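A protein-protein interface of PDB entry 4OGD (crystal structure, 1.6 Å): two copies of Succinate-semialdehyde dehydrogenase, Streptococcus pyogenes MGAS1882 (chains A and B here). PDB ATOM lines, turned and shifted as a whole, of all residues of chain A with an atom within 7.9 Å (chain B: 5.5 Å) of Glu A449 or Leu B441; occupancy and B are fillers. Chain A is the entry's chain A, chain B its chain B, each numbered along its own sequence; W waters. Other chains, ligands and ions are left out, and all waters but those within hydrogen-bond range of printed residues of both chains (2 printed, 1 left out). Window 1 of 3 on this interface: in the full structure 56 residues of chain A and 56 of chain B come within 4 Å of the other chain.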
ATOM      1  N   THR A 106     -29.514   9.758   4.719  1.00  0.00           N
ATOM      2  CA  THR A 106     -28.321   9.124   5.270  1.00  0.00           C
ATOM      3  C   THR A 106     -27.770   9.915   6.450  1.00  0.00           C
ATOM      4  O   THR A 106     -27.221  10.996   6.271  1.00  0.00           O
ATOM      5  CB  THR A 106     -27.215   9.008   4.198  1.00  0.00           C
ATOM      6  OG1 THR A 106     -27.692   8.210   3.110  1.00  0.00           O
ATOM      7  CG2 THR A 106     -25.958   8.366   4.782  1.00  0.00           C
ATOM      8  N   LEU A 108     -25.229  11.150   9.273  1.00  0.00           N
ATOM      9  CA  LEU A 108     -23.788  11.322   9.306  1.00  0.00           C
ATOM     10  C   LEU A 108     -23.316  11.402  10.749  1.00  0.00           C
ATOM     11  O   LEU A 108     -23.854  12.169  11.552  1.00  0.00           O
ATOM     12  CB  LEU A 108     -23.385  12.584   8.549  1.00  0.00           C
ATOM     13  CG  LEU A 108     -23.668  12.591   7.048  1.00  0.00           C
ATOM     14  CD1 LEU A 108     -23.659  14.011   6.497  1.00  0.00           C
ATOM     15  CD2 LEU A 108     -22.637  11.747   6.318  1.00  0.00           C
ATOM     16  N   TYR A 116     -27.113  14.985   8.281  1.00  0.00           N
ATOM     17  CA  TYR A 116     -27.523  13.926   7.358  1.00  0.00           C
ATOM     18  C   TYR A 116     -27.453  14.460   5.938  1.00  0.00           C
ATOM     19  O   TYR A 116     -27.282  15.653   5.726  1.00  0.00           O
ATOM     20  CB  TYR A 116     -28.943  13.432   7.664  1.00  0.00           C
ATOM     21  CG  TYR A 116     -30.010  14.504   7.610  1.00  0.00           C
ATOM     22  CD1 TYR A 116     -30.780  14.689   6.467  1.00  0.00           C
ATOM     23  CD2 TYR A 116     -30.256  15.321   8.712  1.00  0.00           C
ATOM     24  CE1 TYR A 116     -31.769  15.667   6.420  1.00  0.00           C
ATOM     25  CE2 TYR A 116     -31.239  16.294   8.674  1.00  0.00           C
ATOM     26  CZ  TYR A 116     -31.990  16.464   7.531  1.00  0.00           C
ATOM     27  OH  TYR A 116     -32.967  17.438   7.500  1.00  0.00           O
ATOM     28  N   TYR A 117     -27.574  13.583   4.953  1.00  0.00           N
ATOM     29  CA  TYR A 117     -27.759  14.098   3.608  1.00  0.00           C
ATOM     30  C   TYR A 117     -28.914  13.428   2.901  1.00  0.00           C
ATOM     31  O   TYR A 117     -29.183  12.244   3.102  1.00  0.00           O
ATOM     32  CB  TYR A 117     -26.463  14.074   2.775  1.00  0.00           C
ATOM     33  CG  TYR A 117     -25.948  12.715   2.339  1.00  0.00           C
ATOM     34  CD1 TYR A 117     -26.402  12.126   1.163  1.00  0.00           C
ATOM     35  CD2 TYR A 117     -24.967  12.057   3.066  1.00  0.00           C
ATOM     36  CE1 TYR A 117     -25.915  10.903   0.740  1.00  0.00           C
ATOM     37  CE2 TYR A 117     -24.467  10.822   2.642  1.00  0.00           C
ATOM     38  CZ  TYR A 117     -24.959  10.259   1.479  1.00  0.00           C
ATOM     39  OH  TYR A 117     -24.482   9.040   1.033  1.00  0.00           O
ATOM     40  N   LEU A 118     -29.603  14.219   2.091  1.00  0.00           N
ATOM     41  CA  LEU A 118     -30.712  13.726   1.297  1.00  0.00           C
ATOM     42  C   LEU A 118     -30.190  13.324  -0.071  1.00  0.00           C
ATOM     43  O   LEU A 118     -29.101  13.741  -0.476  1.00  0.00           O
ATOM     44  CB  LEU A 118     -31.771  14.817   1.160  1.00  0.00           C
ATOM     45  CG  LEU A 118     -32.297  15.344   2.499  1.00  0.00           C
ATOM     46  CD1 LEU A 118     -33.177  16.556   2.279  1.00  0.00           C
ATOM     47  CD2 LEU A 118     -33.072  14.257   3.237  1.00  0.00           C
ATOM     48  N   LYS A 119     -30.954  12.493  -0.774  1.00  0.00           N
ATOM     49  CA  LYS A 119     -30.632  12.164  -2.155  1.00  0.00           C
ATOM     50  C   LYS A 119     -31.753  12.697  -3.016  1.00  0.00           C
ATOM     51  O   LYS A 119     -32.862  12.165  -3.015  1.00  0.00           O
ATOM     52  CB  LYS A 119     -30.454  10.658  -2.334  1.00  0.00           C
ATOM     53  CG  LYS A 119     -29.201  10.127  -1.663  1.00  0.00           C
ATOM     54  CD  LYS A 119     -29.170   8.604  -1.624  1.00  0.00           C
ATOM     55  CE  LYS A 119     -27.883   8.122  -0.977  1.00  0.00           C
ATOM     56  NZ  LYS A 119     -27.865   6.640  -0.765  1.00  0.00           N
ATOM     57  N   GLN A 120     -31.470  13.777  -3.733  1.00  0.00           N
ATOM     58  CA  GLN A 120     -32.522  14.507  -4.420  1.00  0.00           C
ATOM     59  C   GLN A 120     -32.310  14.540  -5.921  1.00  0.00           C
ATOM     60  O   GLN A 120     -31.177  14.408  -6.405  1.00  0.00           O
ATOM     61  CB  GLN A 120     -32.599  15.936  -3.867  1.00  0.00           C
ATOM     62  CG  GLN A 120     -32.950  15.980  -2.382  1.00  0.00           C
ATOM     63  CD  GLN A 120     -33.122  17.384  -1.873  1.00  0.00           C
ATOM     64  OE1 GLN A 120     -32.236  18.217  -2.027  1.00  0.00           O
ATOM     65  NE2 GLN A 120     -34.281  17.665  -1.281  1.00  0.00           N
ATOM     66  N   SER A 121     -33.399  14.709  -6.665  1.00  0.00           N
ATOM     67  CA  SER A 121     -33.290  14.906  -8.105  1.00  0.00           C
ATOM     68  C   SER A 121     -32.582  16.217  -8.403  1.00  0.00           C
ATOM     69  O   SER A 121     -32.521  17.115  -7.554  1.00  0.00           O
ATOM     70  CB  SER A 121     -34.673  14.917  -8.753  1.00  0.00           C
ATOM     71  OG  SER A 121     -35.438  16.001  -8.244  1.00  0.00           O
ATOM     72  N   THR A 122     -32.054  16.322  -9.616  1.00  0.00           N
ATOM     73  CA  THR A 122     -31.343  17.518 -10.040  1.00  0.00           C
ATOM     74  C   THR A 122     -31.932  18.197 -11.268  1.00  0.00           C
ATOM     75  O   THR A 122     -31.847  19.417 -11.390  1.00  0.00           O
ATOM     76  CB  THR A 122     -29.853  17.224 -10.276  1.00  0.00           C
ATOM     77  OG1 THR A 122     -29.711  16.084 -11.135  1.00  0.00           O
ATOM     78  CG2 THR A 122     -29.171  16.926  -8.953  1.00  0.00           C
ATOM     79  N   LYS A 225     -22.014  17.366 -15.362  1.00  0.00           N
ATOM     80  CA  LYS A 225     -21.511  16.068 -14.899  1.00  0.00           C
ATOM     81  C   LYS A 225     -21.761  14.994 -15.954  1.00  0.00           C
ATOM     82  O   LYS A 225     -22.788  15.011 -16.648  1.00  0.00           O
ATOM     83  CB  LYS A 225     -22.227  15.689 -13.600  1.00  0.00           C
ATOM     84  CG  LYS A 225     -21.609  14.531 -12.820  1.00  0.00           C
ATOM     85  CD  LYS A 225     -22.452  14.241 -11.586  1.00  0.00           C
ATOM     86  CE  LYS A 225     -21.675  13.432 -10.563  1.00  0.00           C
ATOM     87  NZ  LYS A 225     -22.448  13.247  -9.300  1.00  0.00           N
ATOM     88  N   THR A 444     -26.894   6.813  -7.902  1.00  0.00           N
ATOM     89  CA  THR A 444     -26.582   8.156  -7.399  1.00  0.00           C
ATOM     90  C   THR A 444     -25.849   9.082  -8.366  1.00  0.00           C
ATOM     91  O   THR A 444     -25.503  10.201  -7.993  1.00  0.00           O
ATOM     92  CB  THR A 444     -25.789   8.089  -6.095  1.00  0.00           C
ATOM     93  OG1 THR A 444     -24.665   7.229  -6.286  1.00  0.00           O
ATOM     94  CG2 THR A 444     -26.662   7.552  -4.961  1.00  0.00           C
ATOM     95  N   SER A 445     -25.635   8.642  -9.601  1.00  0.00           N
ATOM     96  CA  SER A 445     -24.800   9.404 -10.528  1.00  0.00           C
ATOM     97  C   SER A 445     -25.270  10.835 -10.724  1.00  0.00           C
ATOM     98  O   SER A 445     -24.448  11.753 -10.765  1.00  0.00           O
ATOM     99  CB  SER A 445     -24.727   8.715 -11.886  1.00  0.00           C
ATOM    100  OG  SER A 445     -24.138   7.441 -11.748  1.00  0.00           O
ATOM    101  N   PHE A 446     -26.581  11.022 -10.838  1.00  0.00           N
ATOM    102  CA  PHE A 446     -27.130  12.356 -11.058  1.00  0.00           C
ATOM    103  C   PHE A 446     -28.081  12.792  -9.952  1.00  0.00           C
ATOM    104  O   PHE A 446     -29.055  13.527 -10.182  1.00  0.00           O
ATOM    105  CB  PHE A 446     -27.744  12.454 -12.459  1.00  0.00           C
ATOM    106  CG  PHE A 446     -26.769  12.108 -13.550  1.00  0.00           C
ATOM    107  CD1 PHE A 446     -25.779  13.010 -13.918  1.00  0.00           C
ATOM    108  CD2 PHE A 446     -26.812  10.867 -14.171  1.00  0.00           C
ATOM    109  CE1 PHE A 446     -24.875  12.700 -14.906  1.00  0.00           C
ATOM    110  CE2 PHE A 446     -25.901  10.538 -15.167  1.00  0.00           C
ATOM    111  CZ  PHE A 446     -24.925  11.455 -15.534  1.00  0.00           C
ATOM    112  N   VAL A 447     -27.778  12.346  -8.737  1.00  0.00           N
ATOM    113  CA  VAL A 447     -28.515  12.816  -7.572  1.00  0.00           C
ATOM    114  C   VAL A 447     -27.712  13.872  -6.840  1.00  0.00           C
ATOM    115  O   VAL A 447     -26.473  13.851  -6.842  1.00  0.00           O
ATOM    116  CB  VAL A 447     -28.891  11.679  -6.587  1.00  0.00           C
ATOM    117  CG1 VAL A 447     -29.499  10.492  -7.324  1.00  0.00           C
ATOM    118  CG2 VAL A 447     -27.706  11.265  -5.751  1.00  0.00           C
ATOM    119  N   ASN A 448     -28.432  14.807  -6.235  1.00  0.00           N
ATOM    120  CA  ASN A 448     -27.842  15.818  -5.386  1.00  0.00           C
ATOM    121  C   ASN A 448     -27.782  15.220  -3.997  1.00  0.00           C
ATOM    122  O   ASN A 448     -28.816  15.005  -3.351  1.00  0.00           O
ATOM    123  CB  ASN A 448     -28.725  17.077  -5.400  1.00  0.00           C
ATOM    124  CG  ASN A 448     -28.337  18.087  -4.336  1.00  0.00           C
ATOM    125  OD1 ASN A 448     -27.285  17.973  -3.706  1.00  0.00           O
ATOM    126  ND2 ASN A 448     -29.193  19.094  -4.134  1.00  0.00           N
ATOM    127  N   GLU A 449     -26.571  14.927  -3.556  1.00  0.00           N
ATOM    128  CA  GLU A 449     -26.346  14.498  -2.181  1.00  0.00           C
ATOM    129  C   GLU A 449     -26.308  15.775  -1.355  1.00  0.00           C
ATOM    130  O   GLU A 449     -25.312  16.493  -1.329  1.00  0.00           O
ATOM    131  CB  GLU A 449     -25.059  13.676  -2.077  1.00  0.00           C
ATOM    132  CG  GLU A 449     -25.181  12.318  -2.790  1.00  0.00           C
ATOM    133  CD  GLU A 449     -23.893  11.849  -3.450  1.00  0.00           C
ATOM    134  OE1 GLU A 449     -23.227  12.660  -4.130  1.00  0.00           O
ATOM    135  OE2 GLU A 449     -23.540  10.655  -3.300  1.00  0.00           O
ATOM    136  N   HIS A 450     -27.434  16.070  -0.714  1.00  0.00           N
ATOM    137  CA  HIS A 450     -27.683  17.385  -0.128  1.00  0.00           C
ATOM    138  C   HIS A 450     -27.507  17.318   1.381  1.00  0.00           C
ATOM    139  O   HIS A 450     -28.329  16.719   2.080  1.00  0.00           O
ATOM    140  CB  HIS A 450     -29.117  17.798  -0.489  1.00  0.00           C
ATOM    141  CG  HIS A 450     -29.535  19.149   0.011  1.00  0.00           C
ATOM    142  ND1 HIS A 450     -30.731  19.722  -0.365  1.00  0.00           N
ATOM    143  CD2 HIS A 450     -28.945  20.031   0.857  1.00  0.00           C
ATOM    144  CE1 HIS A 450     -30.863  20.896   0.226  1.00  0.00           C
ATOM    145  NE2 HIS A 450     -29.788  21.113   0.963  1.00  0.00           N
ATOM    146  N   LEU A 451     -26.429  17.926   1.873  1.00  0.00           N
ATOM    147  CA  LEU A 451     -26.117  17.944   3.299  1.00  0.00           C
ATOM    148  C   LEU A 451     -27.044  18.896   4.035  1.00  0.00           C
ATOM    149  O   LEU A 451     -27.250  20.024   3.593  1.00  0.00           O
ATOM    150  CB  LEU A 451     -24.671  18.407   3.517  1.00  0.00           C
ATOM    151  CG  LEU A 451     -24.264  18.760   4.947  1.00  0.00           C
ATOM    152  CD1 LEU A 451     -24.213  17.505   5.808  1.00  0.00           C
ATOM    153  CD2 LEU A 451     -22.900  19.446   4.931  1.00  0.00           C
ATOM    154  N   ILE A 452     -27.601  18.426   5.152  1.00  0.00           N
ATOM    155  CA  ILE A 452     -28.296  19.290   6.108  1.00  0.00           C
ATOM    156  C   ILE A 452     -27.565  19.199   7.439  1.00  0.00           C
ATOM    157  O   ILE A 452     -27.389  18.106   7.992  1.00  0.00           O
ATOM    158  CB  ILE A 452     -29.756  18.859   6.318  1.00  0.00           C
ATOM    159  CG1 ILE A 452     -30.447  18.632   4.976  1.00  0.00           C
ATOM    160  CG2 ILE A 452     -30.491  19.904   7.168  1.00  0.00           C
ATOM    161  CD1 ILE A 452     -30.672  19.884   4.206  1.00  0.00           C
ATOM    162  N   GLY B 410     -26.408  22.091  -2.588  1.00  0.00           N
ATOM    163  CA  GLY B 410     -25.746  20.896  -2.089  1.00  0.00           C
ATOM    164  C   GLY B 410     -25.625  20.844  -0.576  1.00  0.00           C
ATOM    165  O   GLY B 410     -25.399  19.779   0.003  1.00  0.00           O
ATOM    166  N   PRO B 425     -19.906  15.794   3.862  1.00  0.00           N
ATOM    167  CA  PRO B 425     -19.668  15.966   2.424  1.00  0.00           C
ATOM    168  C   PRO B 425     -19.888  17.409   1.996  1.00  0.00           C
ATOM    169  O   PRO B 425     -20.804  18.089   2.485  1.00  0.00           O
ATOM    170  CB  PRO B 425     -20.711  15.042   1.778  1.00  0.00           C
ATOM    171  CG  PRO B 425     -21.833  15.011   2.782  1.00  0.00           C
ATOM    172  CD  PRO B 425     -21.131  15.014   4.124  1.00  0.00           C
ATOM    173  N   GLY B 427     -20.086  19.984  -1.425  1.00  0.00           N
ATOM    174  CA  GLY B 427     -20.171  20.149  -2.866  1.00  0.00           C
ATOM    175  C   GLY B 427     -21.510  20.715  -3.293  1.00  0.00           C
ATOM    176  O   GLY B 427     -22.419  20.882  -2.468  1.00  0.00           O
ATOM    177  N   ARG B 436     -18.499  15.313  -4.700  1.00  0.00           N
ATOM    178  CA  ARG B 436     -18.426  15.694  -3.302  1.00  0.00           C
ATOM    179  C   ARG B 436     -17.018  15.461  -2.769  1.00  0.00           C
ATOM    180  O   ARG B 436     -16.337  14.499  -3.161  1.00  0.00           O
ATOM    181  CB  ARG B 436     -19.442  14.895  -2.474  1.00  0.00           C
ATOM    182  CG  ARG B 436     -20.913  15.165  -2.815  1.00  0.00           C
ATOM    183  CD  ARG B 436     -21.308  16.576  -2.392  1.00  0.00           C
ATOM    184  NE  ARG B 436     -22.705  16.931  -2.664  1.00  0.00           N
ATOM    185  CZ  ARG B 436     -23.131  17.534  -3.772  1.00  0.00           C
ATOM    186  NH1 ARG B 436     -22.280  17.817  -4.753  1.00  0.00           N
ATOM    187  NH2 ARG B 436     -24.408  17.869  -3.898  1.00  0.00           N
ATOM    188  N   LEU B 438     -14.676  15.419   1.022  1.00  0.00           N
ATOM    189  CA  LEU B 438     -14.833  15.077   2.440  1.00  0.00           C
ATOM    190  C   LEU B 438     -15.891  13.998   2.678  1.00  0.00           C
ATOM    191  O   LEU B 438     -16.615  13.594   1.753  1.00  0.00           O
ATOM    192  CB  LEU B 438     -15.066  16.310   3.320  1.00  0.00           C
ATOM    193  CG  LEU B 438     -13.916  17.321   3.250  1.00  0.00           C
ATOM    194  CD1 LEU B 438     -14.215  18.563   4.095  1.00  0.00           C
ATOM    195  CD2 LEU B 438     -12.594  16.665   3.676  1.00  0.00           C
ATOM    196  N   SER B 439     -15.952  13.524   3.921  1.00  0.00           N
ATOM    197  CA  SER B 439     -16.746  12.338   4.284  1.00  0.00           C
ATOM    198  C   SER B 439     -16.313  11.119   3.467  1.00  0.00           C
ATOM    199  O   SER B 439     -15.300  11.153   2.756  1.00  0.00           O
ATOM    200  CB  SER B 439     -18.261  12.592   4.161  1.00  0.00           C
ATOM    201  OG  SER B 439     -18.721  12.509   2.816  1.00  0.00           O
ATOM    202  N   GLU B 440     -17.068  10.033   3.564  1.00  0.00           N
ATOM    203  CA  GLU B 440     -16.738   8.860   2.761  1.00  0.00           C
ATOM    204  C   GLU B 440     -17.077   9.109   1.287  1.00  0.00           C
ATOM    205  O   GLU B 440     -16.497   8.490   0.390  1.00  0.00           O
ATOM    206  CB  GLU B 440     -17.436   7.600   3.288  1.00  0.00           C
ATOM    207  CG  GLU B 440     -16.913   6.337   2.613  1.00  0.00           C
ATOM    208  CD  GLU B 440     -17.398   5.044   3.251  1.00  0.00           C
ATOM    209  OE1 GLU B 440     -18.222   5.092   4.191  1.00  0.00           O
ATOM    210  OE2 GLU B 440     -16.927   3.969   2.814  1.00  0.00           O
ATOM    211  N   LEU B 441     -18.018  10.012   1.031  1.00  0.00           N
ATOM    212  CA  LEU B 441     -18.349  10.365  -0.344  1.00  0.00           C
ATOM    213  C   LEU B 441     -17.124  10.905  -1.077  1.00  0.00           C
ATOM    214  O   LEU B 441     -16.927  10.632  -2.262  1.00  0.00           O
ATOM    215  CB  LEU B 441     -19.488  11.386  -0.398  1.00  0.00           C
ATOM    216  CG  LEU B 441     -20.863  10.912   0.070  1.00  0.00           C
ATOM    217  CD1 LEU B 441     -21.902  11.987  -0.208  1.00  0.00           C
ATOM    218  CD2 LEU B 441     -21.237   9.630  -0.632  1.00  0.00           C
ATOM    219  N   GLY B 442     -16.289  11.652  -0.361  1.00  0.00           N
ATOM    220  CA  GLY B 442     -15.110  12.247  -0.964  1.00  0.00           C
ATOM    221  C   GLY B 442     -13.927  11.299  -0.992  1.00  0.00           C
ATOM    222  O   GLY B 442     -12.819  11.696  -1.355  1.00  0.00           O
ATOM    223  N   PHE B 443     -14.146  10.046  -0.607  1.00  0.00           N
ATOM    224  CA  PHE B 443     -13.068   9.063  -0.647  1.00  0.00           C
ATOM    225  C   PHE B 443     -13.028   8.316  -1.976  1.00  0.00           C
ATOM    226  O   PHE B 443     -11.963   7.856  -2.410  1.00  0.00           O
ATOM    227  CB  PHE B 443     -13.214   8.056   0.491  1.00  0.00           C
ATOM    228  CG  PHE B 443     -12.034   7.124   0.633  1.00  0.00           C
ATOM    229  CD1 PHE B 443     -10.868   7.566   1.241  1.00  0.00           C
ATOM    230  CD2 PHE B 443     -12.100   5.815   0.182  1.00  0.00           C
ATOM    231  CE1 PHE B 443      -9.774   6.722   1.391  1.00  0.00           C
ATOM    232  CE2 PHE B 443     -11.011   4.957   0.323  1.00  0.00           C
ATOM    233  CZ  PHE B 443      -9.843   5.417   0.941  1.00  0.00           C
ATOM    234  N   THR B 444     -14.183   8.179  -2.614  1.00  0.00           N
ATOM    235  CA  THR B 444     -14.289   7.275  -3.751  1.00  0.00           C
ATOM    236  C   THR B 444     -14.268   7.926  -5.142  1.00  0.00           C
ATOM    237  O   THR B 444     -14.406   7.236  -6.144  1.00  0.00           O
ATOM    238  CB  THR B 444     -15.527   6.378  -3.630  1.00  0.00           C
ATOM    239  OG1 THR B 444     -16.688   7.194  -3.473  1.00  0.00           O
ATOM    240  CG2 THR B 444     -15.398   5.447  -2.425  1.00  0.00           C
ATOM    241  N   SER B 445     -14.080   9.239  -5.220  1.00  0.00           N
ATOM    242  CA  SER B 445     -14.132   9.900  -6.530  1.00  0.00           C
ATOM    243  C   SER B 445     -13.229   9.298  -7.603  1.00  0.00           C
ATOM    244  O   SER B 445     -13.643   9.163  -8.762  1.00  0.00           O
ATOM    245  CB  SER B 445     -13.822  11.382  -6.383  1.00  0.00           C
ATOM    246  OG  SER B 445     -14.792  11.964  -5.541  1.00  0.00           O
HETATM  247  O   HOH W   1     -24.283  14.853  -5.482  1.00  0.00           O
HETATM  248  O   HOH W   2     -20.610  12.640  -5.259  1.00  0.00           O
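The backbone carbonyl oxygen of Thr A106 sits at hydrogen-bond distance from the backbone NH of Tyr A117 (2.9 Å). N of Leu A118 is in hydrogen-bond range of O of His A450. N of Asn A448 is in hydrogen-bond range of O of Gln A120 (2.8 Å). A ring nitrogen (ND1) of His A450 is in hydrogen-bond range of the side-chain amide oxygen (OE1) of Gln A120, 2.7 Å away. The side-chain hydroxyl of Ser B439 is in hydrogen-bond range of the backbone NH of Leu B441 (3.1 Å).
Water W1 lies within hydrogen-bond range of O of Val A447 (2.8 Å), OE1 of Glu A449 (2.8 Å) and NH2 of Arg B436 (3.4 Å). Water W2 bridges OE1 of Glu A449 (2.9 Å) and N of Arg B436 (3.5 Å).
Positions printed for both chains: 444 and 445. Of the 10 pairs that touch across the chains among the printed residues, none has its exchanged pair printed and touching as well.
Of the printed residues of chain B, Leu A108 touches Pro B425 (3.6 Å). Printed residues of chain B within 4 Å of Asn A448: Gly B410 and Arg B436. Glu A449 touches just these residues of chain B: Gly B410 (3.5 Å), Arg B436 (3.0 Å) and Leu B441 (3.7 Å). Printed residues of chain B within 4 Å of His A450: Gly B410 (3.3 Å). Of the printed residues of chain A, Gly B410 touches Asn A448 (3.7 Å), Glu A449 (3.5 Å), His A450 (3.3 Å) and Leu A451 (2.8 Å). Of the printed residues of chain A, Arg B436 touches Asn A448 (2.9 Å) and Glu A449 (3.0 Å). Leu B441 touches just these residues of chain A: Tyr A117 and Glu A449. The nearest residue of chain A that does not touch Leu B441 is Leu A108 (6.5 Å).
OD1 of Asn A448 lies within hydrogen-bond range of NH2 of Arg B436 (2.9 Å). NE of Arg B436 is in hydrogen-bond range of O of Glu A449. The backbone carbonyl oxygen of Gly B410 is in hydrogen-bond range of the backbone NH of Leu A451 (2.8 Å).
Of the 12 printed residues of chain B, 4 touch a printed residue of chain A. Of the 19 printed residues of chain A, 6 touch a printed residue of chain B. Hydrophobic or aromatic side chains of chain A that line the printed part of chain B: Leu A108, Tyr A117, His A450 and Leu A451. Among the printed residues, 10 pairs touch across the chains. Among the printed residues, no Asp or Glu carboxylate lies within 4 Å of a Lys or Arg side-chain nitrogen of the other chain.
Among the printed residues, merely in contact across the chains: His A450 with Gly B410 (3.3 Å), Leu A451 with Pro B425 (3.5 Å), Glu A449 with Gly B410 (3.5 Å), Leu A108 with Pro B425 (3.6 Å), Glu A449 with Leu B441 (3.7 Å), Asn A448 with Gly B410 (3.7 Å) and Tyr A117 with Leu B441 (3.7 Å).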
